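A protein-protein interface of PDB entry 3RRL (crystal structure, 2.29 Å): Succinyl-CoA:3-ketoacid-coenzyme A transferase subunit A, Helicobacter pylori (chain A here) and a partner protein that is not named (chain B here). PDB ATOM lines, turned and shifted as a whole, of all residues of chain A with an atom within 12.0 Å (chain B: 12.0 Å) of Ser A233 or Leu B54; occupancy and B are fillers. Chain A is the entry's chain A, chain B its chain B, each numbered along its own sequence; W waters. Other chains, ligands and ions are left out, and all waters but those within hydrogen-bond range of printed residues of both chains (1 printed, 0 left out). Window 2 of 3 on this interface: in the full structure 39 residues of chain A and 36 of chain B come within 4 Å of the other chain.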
ATOM      1  N   ILE A 226      35.343  24.606 -13.825  1.00  0.00           N
ATOM      2  CA  ILE A 226      34.276  24.176 -14.710  1.00  0.00           C
ATOM      3  C   ILE A 226      33.160  25.221 -14.693  1.00  0.00           C
ATOM      4  O   ILE A 226      32.713  25.648 -13.620  1.00  0.00           O
ATOM      5  CB  ILE A 226      33.731  22.807 -14.272  1.00  0.00           C
ATOM      6  CG1 ILE A 226      34.862  21.772 -14.245  1.00  0.00           C
ATOM      7  CG2 ILE A 226      32.597  22.362 -15.178  1.00  0.00           C
ATOM      8  CD1 ILE A 226      34.523  20.498 -13.481  1.00  0.00           C
ATOM      9  N   LYS A 228      30.034  24.782 -16.097  1.00  0.00           N
ATOM     10  CA  LYS A 228      28.826  24.068 -15.705  1.00  0.00           C
ATOM     11  C   LYS A 228      29.080  22.600 -15.438  1.00  0.00           C
ATOM     12  O   LYS A 228      29.377  21.845 -16.358  1.00  0.00           O
ATOM     13  CB  LYS A 228      27.752  24.221 -16.782  1.00  0.00           C
ATOM     14  CG  LYS A 228      27.458  25.666 -17.143  1.00  0.00           C
ATOM     15  CD  LYS A 228      26.663  25.765 -18.434  1.00  0.00           C
ATOM     16  CE  LYS A 228      26.173  27.184 -18.661  1.00  0.00           C
ATOM     17  NZ  LYS A 228      25.151  27.256 -19.743  1.00  0.00           N
ATOM     18  N   ILE A 229      28.912  22.192 -14.187  1.00  0.00           N
ATOM     19  CA  ILE A 229      29.116  20.806 -13.808  1.00  0.00           C
ATOM     20  C   ILE A 229      27.799  20.078 -13.984  1.00  0.00           C
ATOM     21  O   ILE A 229      26.822  20.367 -13.292  1.00  0.00           O
ATOM     22  CB  ILE A 229      29.570  20.690 -12.350  1.00  0.00           C
ATOM     23  CG1 ILE A 229      30.932  21.369 -12.172  1.00  0.00           C
ATOM     24  CG2 ILE A 229      29.611  19.229 -11.915  1.00  0.00           C
ATOM     25  CD1 ILE A 229      31.570  21.159 -10.813  1.00  0.00           C
ATOM     26  N   THR A 230      27.777  19.140 -14.928  1.00  0.00           N
ATOM     27  CA  THR A 230      26.585  18.355 -15.200  1.00  0.00           C
ATOM     28  C   THR A 230      26.860  16.880 -14.976  1.00  0.00           C
ATOM     29  O   THR A 230      27.827  16.337 -15.504  1.00  0.00           O
ATOM     30  CB  THR A 230      26.134  18.549 -16.637  1.00  0.00           C
ATOM     31  OG1 THR A 230      27.254  18.349 -17.507  1.00  0.00           O
ATOM     32  CG2 THR A 230      25.599  19.956 -16.827  1.00  0.00           C
ATOM     33  N   THR A 231      26.010  16.237 -14.183  1.00  0.00           N
ATOM     34  CA  THR A 231      26.183  14.826 -13.877  1.00  0.00           C
ATOM     35  C   THR A 231      24.893  14.062 -14.167  1.00  0.00           C
ATOM     36  O   THR A 231      23.871  14.663 -14.489  1.00  0.00           O
ATOM     37  CB  THR A 231      26.582  14.639 -12.397  1.00  0.00           C
ATOM     38  OG1 THR A 231      25.496  15.027 -11.546  1.00  0.00           O
ATOM     39  CG2 THR A 231      27.787  15.496 -12.066  1.00  0.00           C
ATOM     40  N   ARG A 232      24.927  12.742 -14.019  1.00  0.00           N
ATOM     41  CA  ARG A 232      23.735  11.939 -14.275  1.00  0.00           C
ATOM     42  C   ARG A 232      23.370  11.026 -13.101  1.00  0.00           C
ATOM     43  O   ARG A 232      24.169  10.834 -12.179  1.00  0.00           O
ATOM     44  CB  ARG A 232      23.879  11.137 -15.569  1.00  0.00           C
ATOM     45  CG  ARG A 232      24.774   9.922 -15.467  1.00  0.00           C
ATOM     46  CD  ARG A 232      24.618   9.055 -16.707  1.00  0.00           C
ATOM     47  NE  ARG A 232      25.138   7.711 -16.495  1.00  0.00           N
ATOM     48  CZ  ARG A 232      26.360   7.320 -16.835  1.00  0.00           C
ATOM     49  NH1 ARG A 232      27.196   8.173 -17.413  1.00  0.00           N
ATOM     50  NH2 ARG A 232      26.745   6.075 -16.596  1.00  0.00           N
ATOM     51  N   SER A 233      22.151  10.483 -13.148  1.00  0.00           N
ATOM     52  CA  SER A 233      21.575   9.683 -12.062  1.00  0.00           C
ATOM     53  C   SER A 233      21.226  10.551 -10.862  1.00  0.00           C
ATOM     54  O   SER A 233      20.727  11.665 -11.017  1.00  0.00           O
ATOM     55  CB  SER A 233      22.499   8.532 -11.639  1.00  0.00           C
ATOM     56  OG  SER A 233      22.308   7.387 -12.456  1.00  0.00           O
ATOM     57  N   ASN B  31      18.071  13.704 -26.238  1.00  0.00           N
ATOM     58  CA  ASN B  31      17.315  12.964 -25.232  1.00  0.00           C
ATOM     59  C   ASN B  31      16.197  12.088 -25.805  1.00  0.00           C
ATOM     60  O   ASN B  31      15.750  11.145 -25.158  1.00  0.00           O
ATOM     61  CB  ASN B  31      16.761  13.920 -24.172  1.00  0.00           C
ATOM     62  CG  ASN B  31      17.856  14.707 -23.472  1.00  0.00           C
ATOM     63  OD1 ASN B  31      19.022  14.303 -23.473  1.00  0.00           O
ATOM     64  ND2 ASN B  31      17.488  15.837 -22.870  1.00  0.00           N
ATOM     65  N   GLY B  50      28.749  11.671 -25.387  1.00  0.00           N
ATOM     66  CA  GLY B  50      28.129  10.638 -24.587  1.00  0.00           C
ATOM     67  C   GLY B  50      27.456  11.289 -23.401  1.00  0.00           C
ATOM     68  O   GLY B  50      27.392  12.517 -23.315  1.00  0.00           O
ATOM     69  N   ALA B  51      26.917  10.472 -22.507  1.00  0.00           N
ATOM     70  CA  ALA B  51      26.087  10.972 -21.423  1.00  0.00           C
ATOM     71  C   ALA B  51      26.883  11.859 -20.480  1.00  0.00           C
ATOM     72  O   ALA B  51      28.113  11.857 -20.505  1.00  0.00           O
ATOM     73  CB  ALA B  51      25.472   9.814 -20.663  1.00  0.00           C
ATOM     74  N   TYR B  52      26.176  12.661 -19.691  1.00  0.00           N
ATOM     75  CA  TYR B  52      26.795  13.338 -18.562  1.00  0.00           C
ATOM     76  C   TYR B  52      27.379  12.279 -17.649  1.00  0.00           C
ATOM     77  O   TYR B  52      26.815  11.190 -17.515  1.00  0.00           O
ATOM     78  CB  TYR B  52      25.774  14.174 -17.794  1.00  0.00           C
ATOM     79  CG  TYR B  52      25.181  15.304 -18.601  1.00  0.00           C
ATOM     80  CD1 TYR B  52      25.978  16.106 -19.396  1.00  0.00           C
ATOM     81  CD2 TYR B  52      23.816  15.562 -18.570  1.00  0.00           C
ATOM     82  CE1 TYR B  52      25.441  17.137 -20.139  1.00  0.00           C
ATOM     83  CE2 TYR B  52      23.266  16.593 -19.306  1.00  0.00           C
ATOM     84  CZ  TYR B  52      24.083  17.379 -20.091  1.00  0.00           C
ATOM     85  OH  TYR B  52      23.543  18.407 -20.831  1.00  0.00           O
ATOM     86  N   PRO B  53      28.523  12.588 -17.028  1.00  0.00           N
ATOM     87  CA  PRO B  53      29.217  11.676 -16.113  1.00  0.00           C
ATOM     88  C   PRO B  53      28.476  11.458 -14.795  1.00  0.00           C
ATOM     89  O   PRO B  53      27.735  12.329 -14.332  1.00  0.00           O
ATOM     90  CB  PRO B  53      30.531  12.407 -15.833  1.00  0.00           C
ATOM     91  CG  PRO B  53      30.222  13.839 -16.073  1.00  0.00           C
ATOM     92  CD  PRO B  53      29.259  13.850 -17.213  1.00  0.00           C
ATOM     93  N   LEU B  54      28.681  10.288 -14.199  1.00  0.00           N
ATOM     94  CA  LEU B  54      28.252  10.048 -12.830  1.00  0.00           C
ATOM     95  C   LEU B  54      29.101  10.939 -11.937  1.00  0.00           C
ATOM     96  O   LEU B  54      30.200  11.338 -12.322  1.00  0.00           O
ATOM     97  CB  LEU B  54      28.469   8.584 -12.447  1.00  0.00           C
ATOM     98  CG  LEU B  54      27.729   7.516 -13.258  1.00  0.00           C
ATOM     99  CD1 LEU B  54      28.373   6.137 -13.088  1.00  0.00           C
ATOM    100  CD2 LEU B  54      26.251   7.483 -12.890  1.00  0.00           C
ATOM    101  N   GLU B  55      28.597  11.260 -10.752  1.00  0.00           N
ATOM    102  CA  GLU B  55      29.384  12.019  -9.788  1.00  0.00           C
ATOM    103  C   GLU B  55      30.721  11.313  -9.568  1.00  0.00           C
ATOM    104  O   GLU B  55      30.757  10.100  -9.334  1.00  0.00           O
ATOM    105  CB  GLU B  55      28.624  12.154  -8.464  1.00  0.00           C
ATOM    106  N   GLY B  56      31.817  12.061  -9.665  1.00  0.00           N
ATOM    107  CA  GLY B  56      33.135  11.494  -9.443  1.00  0.00           C
ATOM    108  C   GLY B  56      33.877  11.161 -10.723  1.00  0.00           C
ATOM    109  O   GLY B  56      35.100  11.008 -10.723  1.00  0.00           O
ATOM    110  N   SER B  57      33.129  11.018 -11.812  1.00  0.00           N
ATOM    111  CA  SER B  57      33.712  10.871 -13.141  1.00  0.00           C
ATOM    112  C   SER B  57      33.772  12.217 -13.863  1.00  0.00           C
ATOM    113  O   SER B  57      34.104  12.286 -15.046  1.00  0.00           O
ATOM    114  CB  SER B  57      32.945   9.837 -13.973  1.00  0.00           C
ATOM    115  OG  SER B  57      33.268   8.515 -13.567  1.00  0.00           O
ATOM    116  N   VAL B  58      33.413  13.279 -13.147  1.00  0.00           N
ATOM    117  CA  VAL B  58      33.505  14.638 -13.669  1.00  0.00           C
ATOM    118  C   VAL B  58      34.939  14.971 -14.075  1.00  0.00           C
ATOM    119  O   VAL B  58      35.870  14.768 -13.301  1.00  0.00           O
ATOM    120  CB  VAL B  58      33.033  15.666 -12.625  1.00  0.00           C
ATOM    121  CG1 VAL B  58      33.144  17.073 -13.182  1.00  0.00           C
ATOM    122  CG2 VAL B  58      31.600  15.367 -12.205  1.00  0.00           C
ATOM    123  N   ASP B  59      35.118  15.467 -15.294  1.00  0.00           N
ATOM    124  CA  ASP B  59      36.457  15.790 -15.793  1.00  0.00           C
ATOM    125  C   ASP B  59      36.426  17.136 -16.509  1.00  0.00           C
ATOM    126  O   ASP B  59      35.766  17.279 -17.533  1.00  0.00           O
ATOM    127  CB  ASP B  59      36.932  14.684 -16.738  1.00  0.00           C
ATOM    128  CG  ASP B  59      38.365  14.881 -17.216  1.00  0.00           C
ATOM    129  OD1 ASP B  59      38.931  15.981 -17.016  1.00  0.00           O
ATOM    130  OD2 ASP B  59      38.919  13.931 -17.814  1.00  0.00           O
ATOM    131  N   ALA B  60      37.149  18.114 -15.974  1.00  0.00           N
ATOM    132  CA  ALA B  60      37.115  19.475 -16.506  1.00  0.00           C
ATOM    133  C   ALA B  60      37.645  19.548 -17.935  1.00  0.00           C
ATOM    134  O   ALA B  60      37.247  20.423 -18.706  1.00  0.00           O
ATOM    135  CB  ALA B  60      37.914  20.408 -15.612  1.00  0.00           C
ATOM    136  N   LEU B  62      37.024  17.580 -20.217  1.00  0.00           N
ATOM    137  CA  LEU B  62      36.072  17.014 -21.160  1.00  0.00           C
ATOM    138  C   LEU B  62      34.705  17.699 -21.096  1.00  0.00           C
ATOM    139  O   LEU B  62      33.919  17.465 -20.176  1.00  0.00           O
ATOM    140  CB  LEU B  62      35.941  15.514 -20.893  1.00  0.00           C
ATOM    141  CG  LEU B  62      34.982  14.701 -21.756  1.00  0.00           C
ATOM    142  CD1 LEU B  62      35.285  14.907 -23.232  1.00  0.00           C
ATOM    143  CD2 LEU B  62      35.072  13.227 -21.364  1.00  0.00           C
ATOM    144  N   GLU B  68      29.657  22.206 -20.794  1.00  0.00           N
ATOM    145  CA  GLU B  68      29.144  21.240 -19.828  1.00  0.00           C
ATOM    146  C   GLU B  68      30.051  20.017 -19.755  1.00  0.00           C
ATOM    147  O   GLU B  68      30.611  19.587 -20.768  1.00  0.00           O
ATOM    148  CB  GLU B  68      27.739  20.798 -20.218  1.00  0.00           C
ATOM    149  CG  GLU B  68      26.764  21.946 -20.408  1.00  0.00           C
ATOM    150  CD  GLU B  68      25.368  21.469 -20.781  1.00  0.00           C
ATOM    151  OE1 GLU B  68      25.256  20.419 -21.452  1.00  0.00           O
ATOM    152  OE2 GLU B  68      24.383  22.145 -20.399  1.00  0.00           O
ATOM    153  N   THR B  69      30.195  19.452 -18.560  1.00  0.00           N
ATOM    154  CA  THR B  69      31.003  18.249 -18.403  1.00  0.00           C
ATOM    155  C   THR B  69      30.265  17.039 -18.952  1.00  0.00           C
ATOM    156  O   THR B  69      29.080  16.831 -18.651  1.00  0.00           O
ATOM    157  CB  THR B  69      31.368  17.996 -16.930  1.00  0.00           C
ATOM    158  OG1 THR B  69      30.170  17.919 -16.146  1.00  0.00           O
ATOM    159  CG2 THR B  69      32.252  19.119 -16.411  1.00  0.00           C
ATOM    160  N   ILE B  70      30.968  16.235 -19.747  1.00  0.00           N
ATOM    161  CA  ILE B  70      30.354  15.087 -20.419  1.00  0.00           C
ATOM    162  C   ILE B  70      31.238  13.851 -20.355  1.00  0.00           C
ATOM    163  O   ILE B  70      32.287  13.861 -19.718  1.00  0.00           O
ATOM    164  CB  ILE B  70      30.082  15.384 -21.906  1.00  0.00           C
ATOM    165  CG1 ILE B  70      31.377  15.798 -22.606  1.00  0.00           C
ATOM    166  CG2 ILE B  70      29.035  16.476 -22.048  1.00  0.00           C
ATOM    167  CD1 ILE B  70      31.248  15.907 -24.129  1.00  0.00           C
ATOM    168  N   THR B  71      30.804  12.789 -21.025  1.00  0.00           N
ATOM    169  CA  THR B  71      31.660  11.630 -21.255  1.00  0.00           C
ATOM    170  C   THR B  71      31.729  11.355 -22.751  1.00  0.00           C
ATOM    171  O   THR B  71      31.155  12.096 -23.551  1.00  0.00           O
ATOM    172  CB  THR B  71      31.142  10.375 -20.542  1.00  0.00           C
ATOM    173  OG1 THR B  71      29.883   9.990 -21.112  1.00  0.00           O
ATOM    174  CG2 THR B  71      30.980  10.634 -19.038  1.00  0.00           C
ATOM    175  N   VAL B  72      32.439  10.296 -23.125  1.00  0.00           N
ATOM    176  CA  VAL B  72      32.538   9.896 -24.520  1.00  0.00           C
ATOM    177  C   VAL B  72      32.032   8.472 -24.675  1.00  0.00           C
ATOM    178  O   VAL B  72      32.086   7.686 -23.729  1.00  0.00           O
ATOM    179  CB  VAL B  72      33.997   9.975 -25.034  1.00  0.00           C
ATOM    180  CG1 VAL B  72      34.513  11.393 -24.944  1.00  0.00           C
ATOM    181  CG2 VAL B  72      34.897   9.048 -24.241  1.00  0.00           C
HETATM  182  O   HOH W   1      30.200   8.304 -15.875  1.00  0.00           O
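The side-chain hydroxyl (OH) of Tyr B52 sits at hydrogen-bond distance from the side-chain carboxylate (OE1) of Glu B68 (2.7 Å).
Printed residues of chain B within 4 Å of Lys A228: Glu B68 (3.5 Å) and Thr B69 (3.4 Å).
Printed residues of chain B within 4 Å of Thr A230: Tyr B52 (3.2 Å), Pro B53 (3.3 Å), Glu B68 (3.7 Å) and Thr B69 (2.6 Å).
Of chain B, only Tyr B52, Pro B53 and Val B58 come within 4 Å of Thr A231.
Printed residues of chain B within 4 Å of Arg A232: Tyr B52, Pro B53 and Leu B54.
Ser A233 touches just one residue of chain B: Leu B54.
Ala B51 touches none of the printed residues of chain A.
Leu B54 touches just these residues of chain A: Arg A232 (3.8 Å) and Ser A233 (3.97 Å).
No residue of chain A comes within 4 Å of Gly B56.
Val B58 touches two residues of chain A.
Asp B59 touches none of the printed residues of chain A.
Of the printed residues of chain A, Ala B60 touches Ile A226.
Printed residues of chain A within 4 Å of Glu B68: Lys A228 and Thr A230.
The nearest residue of chain B that does not touch Ser A233 is Pro B53 (6.0 Å).
Water W1 bridges N of Leu B54 and NH1 of Arg A232.
Val B58 touches Ile A226.
Ala B60 touches Ile A226.
CG2 of Thr B69 touches CG2 of Ile A226, 3.5 Å away.
Lys A228 touches Glu B68 (O to CA, 3.5 Å).
Thr A230 touches Tyr B52 (OG1 to CD1, 3.2 Å).
Pro B53 touches Thr A230 (CD to O, 3.3 Å).
OG1 of Thr A230 touches CB of Glu B68, at 3.7 Å.
C of Thr A231 touches CB of Tyr B52, at 3.7 Å.
CG2 of Thr A231 touches CG2 of Val B58, 3.8 Å away.
Arg A232 touches Leu B54.
The backbone NH of Thr B69 lies within hydrogen-bond range of the backbone carbonyl oxygen of Lys A228 (3.4 Å).
OG1 of Thr A230 lies within hydrogen-bond range of O of Thr B69 (2.6 Å).
The guanidinium group (NH1) of Arg A232 lies within hydrogen-bond range of the backbone carbonyl oxygen (O) of Tyr B52 (3.0 Å).
The backbone NH (N) of Arg A232 lies within hydrogen-bond range of the backbone carbonyl oxygen (O) of Pro B53 (2.9 Å).
Hydrophobic or aromatic side chains of chain B within 4 Å of the printed part of chain A: Tyr B52, Pro B53, Leu B54, Val B58 and Ala B60.
Hydrophobic or aromatic side chains of chain A that line the printed part of chain B: Ile A226.
Among the printed residues, 17 pairs touch across the chains.
Among the printed residues, no Asp or Glu carboxylate lies within 4 Å of a Lys or Arg side-chain nitrogen of the other chain.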
